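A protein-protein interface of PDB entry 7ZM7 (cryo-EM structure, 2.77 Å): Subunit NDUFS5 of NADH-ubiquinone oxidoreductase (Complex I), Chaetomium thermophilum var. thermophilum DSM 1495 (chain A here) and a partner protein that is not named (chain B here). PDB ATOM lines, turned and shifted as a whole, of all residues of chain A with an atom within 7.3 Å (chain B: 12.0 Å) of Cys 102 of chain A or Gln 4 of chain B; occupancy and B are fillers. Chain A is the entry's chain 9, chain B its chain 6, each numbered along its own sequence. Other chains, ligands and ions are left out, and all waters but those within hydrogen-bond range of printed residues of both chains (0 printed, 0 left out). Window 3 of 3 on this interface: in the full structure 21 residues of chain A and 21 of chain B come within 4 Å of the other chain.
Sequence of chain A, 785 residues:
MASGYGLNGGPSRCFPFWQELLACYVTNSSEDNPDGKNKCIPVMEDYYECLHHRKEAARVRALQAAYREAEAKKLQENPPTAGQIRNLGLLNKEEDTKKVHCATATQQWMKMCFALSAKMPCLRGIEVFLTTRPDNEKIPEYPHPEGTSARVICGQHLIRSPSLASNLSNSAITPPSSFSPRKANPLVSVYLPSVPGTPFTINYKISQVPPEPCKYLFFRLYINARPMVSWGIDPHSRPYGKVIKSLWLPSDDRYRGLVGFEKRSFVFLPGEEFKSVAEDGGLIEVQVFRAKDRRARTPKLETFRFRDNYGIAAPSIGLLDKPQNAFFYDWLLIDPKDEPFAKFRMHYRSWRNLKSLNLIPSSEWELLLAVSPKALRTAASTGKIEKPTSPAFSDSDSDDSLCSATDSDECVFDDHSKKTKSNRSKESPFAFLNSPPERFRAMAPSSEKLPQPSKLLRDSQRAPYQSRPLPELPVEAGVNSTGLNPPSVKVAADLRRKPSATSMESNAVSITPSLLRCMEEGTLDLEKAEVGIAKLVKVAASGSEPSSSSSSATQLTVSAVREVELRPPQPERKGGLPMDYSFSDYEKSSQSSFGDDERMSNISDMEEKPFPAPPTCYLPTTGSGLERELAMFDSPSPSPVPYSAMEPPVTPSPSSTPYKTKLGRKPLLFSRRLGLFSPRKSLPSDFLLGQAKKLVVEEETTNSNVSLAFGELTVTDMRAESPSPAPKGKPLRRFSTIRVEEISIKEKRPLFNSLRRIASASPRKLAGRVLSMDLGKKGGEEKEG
SG of Cys 102 of chain A is in hydrogen-bond range of O of Lys 99 of chain A (3.8 Å).
CG of Glu 71 of chain A touches CG2 of Ile 5 of chain B, 3.5 Å away. Lys 74 of chain A touches Ser 3 of chain B (NZ to O, 3.96 Å). Val 100 of chain A touches Leu 8 of chain B. SG of Cys 102 of chain A touches CB of Gln 4 of chain B, at 3.5 Å.
Cys 102 of chain A touches one residue of chain B. Gln 4 of chain B touches just one residue of chain A: Cys 102 (3.5 Å). No residue of chain B comes within 4 Å of Lys 99 of chain A. No residue of chain B comes within 4 Å of His 101 of chain A. No residue of chain B comes within 4 Å of Ala 103 of chain A. Printed residues of chain A within 4 Å of Ser 3 of chain B: Lys 74. Of the printed residues of chain B, Glu 71 of chain A touches Ile 5 (3.5 Å). Of the printed residues of chain A, Ile 5 of chain B touches Glu 71. Printed residues of chain B within 4 Å of Lys 74 of chain A: Ser 3. Of the printed residues of chain A, Leu 8 of chain B touches Val 100 (3.8 Å). The nearest residue of chain B that does not touch Cys 102 of chain A is Ser 3 of chain B (4.4 Å).
Hydrophobic or aromatic side chains of chain B within 4 Å of the printed part of chain A: Ile 5 and Leu 8. Along chain B the printed residues that touch a printed residue of chain A span positions 3 to 8. Of the 14 printed residues of chain A, 4 touch a printed residue of chain B. Hydrophobic or aromatic side chains of chain A within 4 Å of the printed part of chain B: Val 100. Among the printed residues, 4 pairs touch across the chains. Among the printed residues, no Asp or Glu carboxylate lies within 4 Å of a Lys or Arg side-chain nitrogen of the other chain.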
ATOM      1  N   GLU A  71      21.249 -19.315 -22.476  1.00  0.00           N
ATOM      2  CA  GLU A  71      20.271 -19.728 -23.473  1.00  0.00           C
ATOM      3  C   GLU A  71      19.408 -18.581 -23.977  1.00  0.00           C
ATOM      4  O   GLU A  71      18.358 -18.831 -24.570  1.00  0.00           O
ATOM      5  CB  GLU A  71      19.387 -20.850 -22.913  1.00  0.00           C
ATOM      6  CG  GLU A  71      19.944 -22.251 -23.135  1.00  0.00           C
ATOM      7  CD  GLU A  71      21.075 -22.607 -22.192  1.00  0.00           C
ATOM      8  OE1 GLU A  71      21.467 -21.749 -21.381  1.00  0.00           O
ATOM      9  OE2 GLU A  71      21.567 -23.753 -22.257  1.00  0.00           O
ATOM     10  N   LYS A  74      22.224 -17.685 -27.558  1.00  0.00           N
ATOM     11  CA  LYS A  74      22.567 -18.693 -28.546  1.00  0.00           C
ATOM     12  C   LYS A  74      21.447 -18.830 -29.572  1.00  0.00           C
ATOM     13  O   LYS A  74      20.281 -18.529 -29.306  1.00  0.00           O
ATOM     14  CB  LYS A  74      22.837 -20.038 -27.877  1.00  0.00           C
ATOM     15  CG  LYS A  74      21.594 -20.849 -27.586  1.00  0.00           C
ATOM     16  CD  LYS A  74      21.939 -22.093 -26.793  1.00  0.00           C
ATOM     17  CE  LYS A  74      22.843 -23.016 -27.583  1.00  0.00           C
ATOM     18  NZ  LYS A  74      23.130 -24.269 -26.836  1.00  0.00           N
ATOM     19  N   GLU A  77      17.223 -23.199 -33.143  1.00  0.00           N
ATOM     20  CA  GLU A  77      16.898 -23.803 -34.430  1.00  0.00           C
ATOM     21  C   GLU A  77      15.395 -24.004 -34.584  1.00  0.00           C
ATOM     22  O   GLU A  77      14.761 -23.408 -35.460  1.00  0.00           O
ATOM     23  CB  GLU A  77      17.640 -25.132 -34.583  1.00  0.00           C
ATOM     24  CG  GLU A  77      19.093 -25.081 -34.139  1.00  0.00           C
ATOM     25  CD  GLU A  77      19.931 -24.145 -34.985  1.00  0.00           C
ATOM     26  OE1 GLU A  77      19.651 -24.023 -36.196  1.00  0.00           O
ATOM     27  OE2 GLU A  77      20.869 -23.529 -34.439  1.00  0.00           O
ATOM     28  N   ASN A  78      14.810 -24.834 -33.727  1.00  0.00           N
ATOM     29  CA  ASN A  78      13.388 -25.140 -33.778  1.00  0.00           C
ATOM     30  C   ASN A  78      12.910 -25.558 -32.395  1.00  0.00           C
ATOM     31  O   ASN A  78      13.091 -26.717 -31.999  1.00  0.00           O
ATOM     32  CB  ASN A  78      13.108 -26.246 -34.796  1.00  0.00           C
ATOM     33  CG  ASN A  78      12.926 -25.712 -36.199  1.00  0.00           C
ATOM     34  OD1 ASN A  78      12.237 -24.716 -36.412  1.00  0.00           O
ATOM     35  ND2 ASN A  78      13.545 -26.374 -37.167  1.00  0.00           N
ATOM     36  N   PRO A  79      12.306 -24.656 -31.632  1.00  0.00           N
ATOM     37  CA  PRO A  79      11.871 -25.002 -30.280  1.00  0.00           C
ATOM     38  C   PRO A  79      10.733 -26.003 -30.319  1.00  0.00           C
ATOM     39  O   PRO A  79       9.736 -25.802 -31.029  1.00  0.00           O
ATOM     40  CB  PRO A  79      11.412 -23.656 -29.703  1.00  0.00           C
ATOM     41  CG  PRO A  79      11.030 -22.854 -30.896  1.00  0.00           C
ATOM     42  CD  PRO A  79      11.967 -23.269 -31.991  1.00  0.00           C
ATOM     43  N   PRO A  80      10.847 -27.101 -29.577  1.00  0.00           N
ATOM     44  CA  PRO A  80       9.771 -28.097 -29.570  1.00  0.00           C
ATOM     45  C   PRO A  80       8.540 -27.563 -28.860  1.00  0.00           C
ATOM     46  O   PRO A  80       8.627 -26.988 -27.775  1.00  0.00           O
ATOM     47  CB  PRO A  80      10.386 -29.277 -28.809  1.00  0.00           C
ATOM     48  CG  PRO A  80      11.866 -29.023 -28.826  1.00  0.00           C
ATOM     49  CD  PRO A  80      12.006 -27.541 -28.790  1.00  0.00           C
ATOM     50  N   ASP A  96       8.040 -37.575 -32.832  1.00  0.00           N
ATOM     51  CA  ASP A  96       8.156 -36.467 -31.890  1.00  0.00           C
ATOM     52  C   ASP A  96       9.308 -36.661 -30.916  1.00  0.00           C
ATOM     53  O   ASP A  96      10.000 -35.694 -30.589  1.00  0.00           O
ATOM     54  CB  ASP A  96       6.848 -36.274 -31.129  1.00  0.00           C
ATOM     55  CG  ASP A  96       5.855 -35.421 -31.890  1.00  0.00           C
ATOM     56  OD1 ASP A  96       6.295 -34.606 -32.727  1.00  0.00           O
ATOM     57  OD2 ASP A  96       4.639 -35.559 -31.645  1.00  0.00           O
ATOM     58  N   THR A  97       9.531 -37.888 -30.447  1.00  0.00           N
ATOM     59  CA  THR A  97      10.622 -38.120 -29.512  1.00  0.00           C
ATOM     60  C   THR A  97      11.975 -37.860 -30.151  1.00  0.00           C
ATOM     61  O   THR A  97      12.870 -37.319 -29.496  1.00  0.00           O
ATOM     62  CB  THR A  97      10.567 -39.545 -28.974  1.00  0.00           C
ATOM     63  OG1 THR A  97      10.941 -40.457 -30.012  1.00  0.00           O
ATOM     64  CG2 THR A  97       9.180 -39.868 -28.520  1.00  0.00           C
ATOM     65  N   LYS A  98      12.155 -38.243 -31.412  1.00  0.00           N
ATOM     66  CA  LYS A  98      13.421 -37.949 -32.072  1.00  0.00           C
ATOM     67  C   LYS A  98      13.646 -36.450 -32.192  1.00  0.00           C
ATOM     68  O   LYS A  98      14.776 -35.977 -32.038  1.00  0.00           O
ATOM     69  CB  LYS A  98      13.474 -38.611 -33.447  1.00  0.00           C
ATOM     70  CG  LYS A  98      14.165 -39.963 -33.443  1.00  0.00           C
ATOM     71  CD  LYS A  98      14.160 -40.589 -34.825  1.00  0.00           C
ATOM     72  CE  LYS A  98      14.239 -42.105 -34.744  1.00  0.00           C
ATOM     73  NZ  LYS A  98      14.558 -42.714 -36.064  1.00  0.00           N
ATOM     74  N   LYS A  99      12.586 -35.689 -32.465  1.00  0.00           N
ATOM     75  CA  LYS A  99      12.726 -34.239 -32.527  1.00  0.00           C
ATOM     76  C   LYS A  99      13.105 -33.663 -31.170  1.00  0.00           C
ATOM     77  O   LYS A  99      13.918 -32.737 -31.089  1.00  0.00           O
ATOM     78  CB  LYS A  99      11.437 -33.606 -33.037  1.00  0.00           C
ATOM     79  CG  LYS A  99      11.498 -32.097 -33.138  1.00  0.00           C
ATOM     80  CD  LYS A  99      12.646 -31.662 -34.028  1.00  0.00           C
ATOM     81  CE  LYS A  99      12.423 -32.080 -35.471  1.00  0.00           C
ATOM     82  NZ  LYS A  99      13.554 -31.654 -36.341  1.00  0.00           N
ATOM     83  N   VAL A 100      12.522 -34.190 -30.094  1.00  0.00           N
ATOM     84  CA  VAL A 100      12.811 -33.648 -28.774  1.00  0.00           C
ATOM     85  C   VAL A 100      14.265 -33.895 -28.396  1.00  0.00           C
ATOM     86  O   VAL A 100      14.945 -33.008 -27.867  1.00  0.00           O
ATOM     87  CB  VAL A 100      11.850 -34.238 -27.733  1.00  0.00           C
ATOM     88  CG1 VAL A 100      12.233 -33.758 -26.354  1.00  0.00           C
ATOM     89  CG2 VAL A 100      10.428 -33.835 -28.042  1.00  0.00           C
ATOM     90  N   HIS A 101      14.764 -35.105 -28.666  1.00  0.00           N
ATOM     91  CA  HIS A 101      16.138 -35.469 -28.220  1.00  0.00           C
ATOM     92  C   HIS A 101      17.200 -35.123 -29.268  1.00  0.00           C
ATOM     93  O   HIS A 101      18.382 -35.426 -29.004  1.00  0.00           O
ATOM     94  CB  HIS A 101      16.185 -36.947 -27.814  1.00  0.00           C
ATOM     95  CG  HIS A 101      15.138 -37.308 -26.817  1.00  0.00           C
ATOM     96  ND1 HIS A 101      15.014 -36.646 -25.613  1.00  0.00           N
ATOM     97  CD2 HIS A 101      14.172 -38.250 -26.835  1.00  0.00           C
ATOM     98  CE1 HIS A 101      14.012 -37.163 -24.933  1.00  0.00           C
ATOM     99  NE2 HIS A 101      13.480 -38.151 -25.661  1.00  0.00           N
ATOM    100  N   CYS A 102      16.807 -34.533 -30.400  1.00  0.00           N
ATOM    101  CA  CYS A 102      17.762 -34.110 -31.423  1.00  0.00           C
ATOM    102  C   CYS A 102      18.743 -35.229 -31.760  1.00  0.00           C
ATOM    103  O   CYS A 102      19.948 -35.011 -31.899  1.00  0.00           O
ATOM    104  CB  CYS A 102      18.501 -32.841 -30.994  1.00  0.00           C
ATOM    105  SG  CYS A 102      17.433 -31.396 -30.806  1.00  0.00           S
ATOM    106  N   ALA A 103      18.220 -36.442 -31.890  1.00  0.00           N
ATOM    107  CA  ALA A 103      19.036 -37.587 -32.268  1.00  0.00           C
ATOM    108  C   ALA A 103      18.850 -37.899 -33.747  1.00  0.00           C
ATOM    109  O   ALA A 103      18.196 -37.148 -34.470  1.00  0.00           O
ATOM    110  CB  ALA A 103      18.685 -38.794 -31.419  1.00  0.00           C
ATOM    111  N   SER B   3      21.904 -30.482 -28.132  1.00  0.00           N
ATOM    112  CA  SER B   3      21.806 -29.311 -29.044  1.00  0.00           C
ATOM    113  C   SER B   3      20.658 -28.405 -28.590  1.00  0.00           C
ATOM    114  O   SER B   3      20.930 -27.237 -28.251  1.00  0.00           O
ATOM    115  CB  SER B   3      21.622 -29.754 -30.471  1.00  0.00           C
ATOM    116  N   GLN B   4      19.428 -28.928 -28.580  1.00  0.00           N
ATOM    117  CA  GLN B   4      18.259 -28.143 -28.101  1.00  0.00           C
ATOM    118  C   GLN B   4      18.345 -28.023 -26.578  1.00  0.00           C
ATOM    119  O   GLN B   4      19.051 -28.849 -25.965  1.00  0.00           O
ATOM    120  CB  GLN B   4      16.946 -28.804 -28.520  1.00  0.00           C
ATOM    121  N   ILE B   5      17.649 -27.047 -25.991  1.00  0.00           N
ATOM    122  CA  ILE B   5      17.800 -26.833 -24.523  1.00  0.00           C
ATOM    123  C   ILE B   5      17.418 -28.133 -23.803  1.00  0.00           C
ATOM    124  O   ILE B   5      16.342 -28.685 -24.097  1.00  0.00           O
ATOM    125  CB  ILE B   5      16.954 -25.623 -24.075  1.00  0.00           C
ATOM    126  CG1 ILE B   5      15.478 -25.771 -24.457  1.00  0.00           C
ATOM    127  CG2 ILE B   5      17.534 -24.338 -24.641  1.00  0.00           C
ATOM    128  CD1 ILE B   5      14.613 -24.610 -24.027  1.00  0.00           C
ATOM    129  N   SER B   6      18.295 -28.625 -22.923  1.00  0.00           N
ATOM    130  CA  SER B   6      18.042 -29.911 -22.224  1.00  0.00           C
ATOM    131  C   SER B   6      16.890 -29.776 -21.231  1.00  0.00           C
ATOM    132  O   SER B   6      16.078 -30.706 -21.144  1.00  0.00           O
ATOM    133  CB  SER B   6      19.279 -30.444 -21.597  1.00  0.00           C
ATOM    134  OG  SER B   6      20.231 -30.796 -22.589  1.00  0.00           O
ATOM    135  N   LEU B   7      16.839 -28.658 -20.507  1.00  0.00           N
ATOM    136  CA  LEU B   7      15.724 -28.416 -19.559  1.00  0.00           C
ATOM    137  C   LEU B   7      14.498 -28.017 -20.371  1.00  0.00           C
ATOM    138  O   LEU B   7      14.634 -27.128 -21.214  1.00  0.00           O
ATOM    139  CB  LEU B   7      16.128 -27.308 -18.586  1.00  0.00           C
ATOM    140  CG  LEU B   7      17.265 -27.634 -17.625  1.00  0.00           C
ATOM    141  CD1 LEU B   7      17.628 -26.402 -16.809  1.00  0.00           C
ATOM    142  CD2 LEU B   7      16.883 -28.787 -16.709  1.00  0.00           C
ATOM    143  N   LEU B   8      13.351 -28.646 -20.111  1.00  0.00           N
ATOM    144  CA  LEU B   8      12.108 -28.390 -20.879  1.00  0.00           C
ATOM    145  C   LEU B   8      10.961 -28.015 -19.936  1.00  0.00           C
ATOM    146  O   LEU B   8      10.706 -28.773 -19.001  1.00  0.00           O
ATOM    147  CB  LEU B   8      11.786 -29.641 -21.699  1.00  0.00           C
ATOM    148  CG  LEU B   8      12.593 -29.812 -22.983  1.00  0.00           C
ATOM    149  CD1 LEU B   8      11.969 -30.886 -23.856  1.00  0.00           C
ATOM    150  CD2 LEU B   8      12.671 -28.500 -23.746  1.00  0.00           C
ATOM    151  N   LEU B   9      10.324 -26.917 -20.098  1.00  0.00           N
ATOM    152  CA  LEU B   9       9.228 -26.472 -19.202  1.00  0.00           C
ATOM    153  C   LEU B   9       7.927 -26.448 -20.002  1.00  0.00           C
ATOM    154  O   LEU B   9       7.897 -25.771 -21.044  1.00  0.00           O
ATOM    155  CB  LEU B   9       9.569 -25.067 -18.698  1.00  0.00           C
ATOM    156  CG  LEU B   9       8.709 -24.542 -17.550  1.00  0.00           C
ATOM    157  CD1 LEU B   9       8.803 -25.462 -16.344  1.00  0.00           C
ATOM    158  CD2 LEU B   9       9.130 -23.132 -17.172  1.00  0.00           C
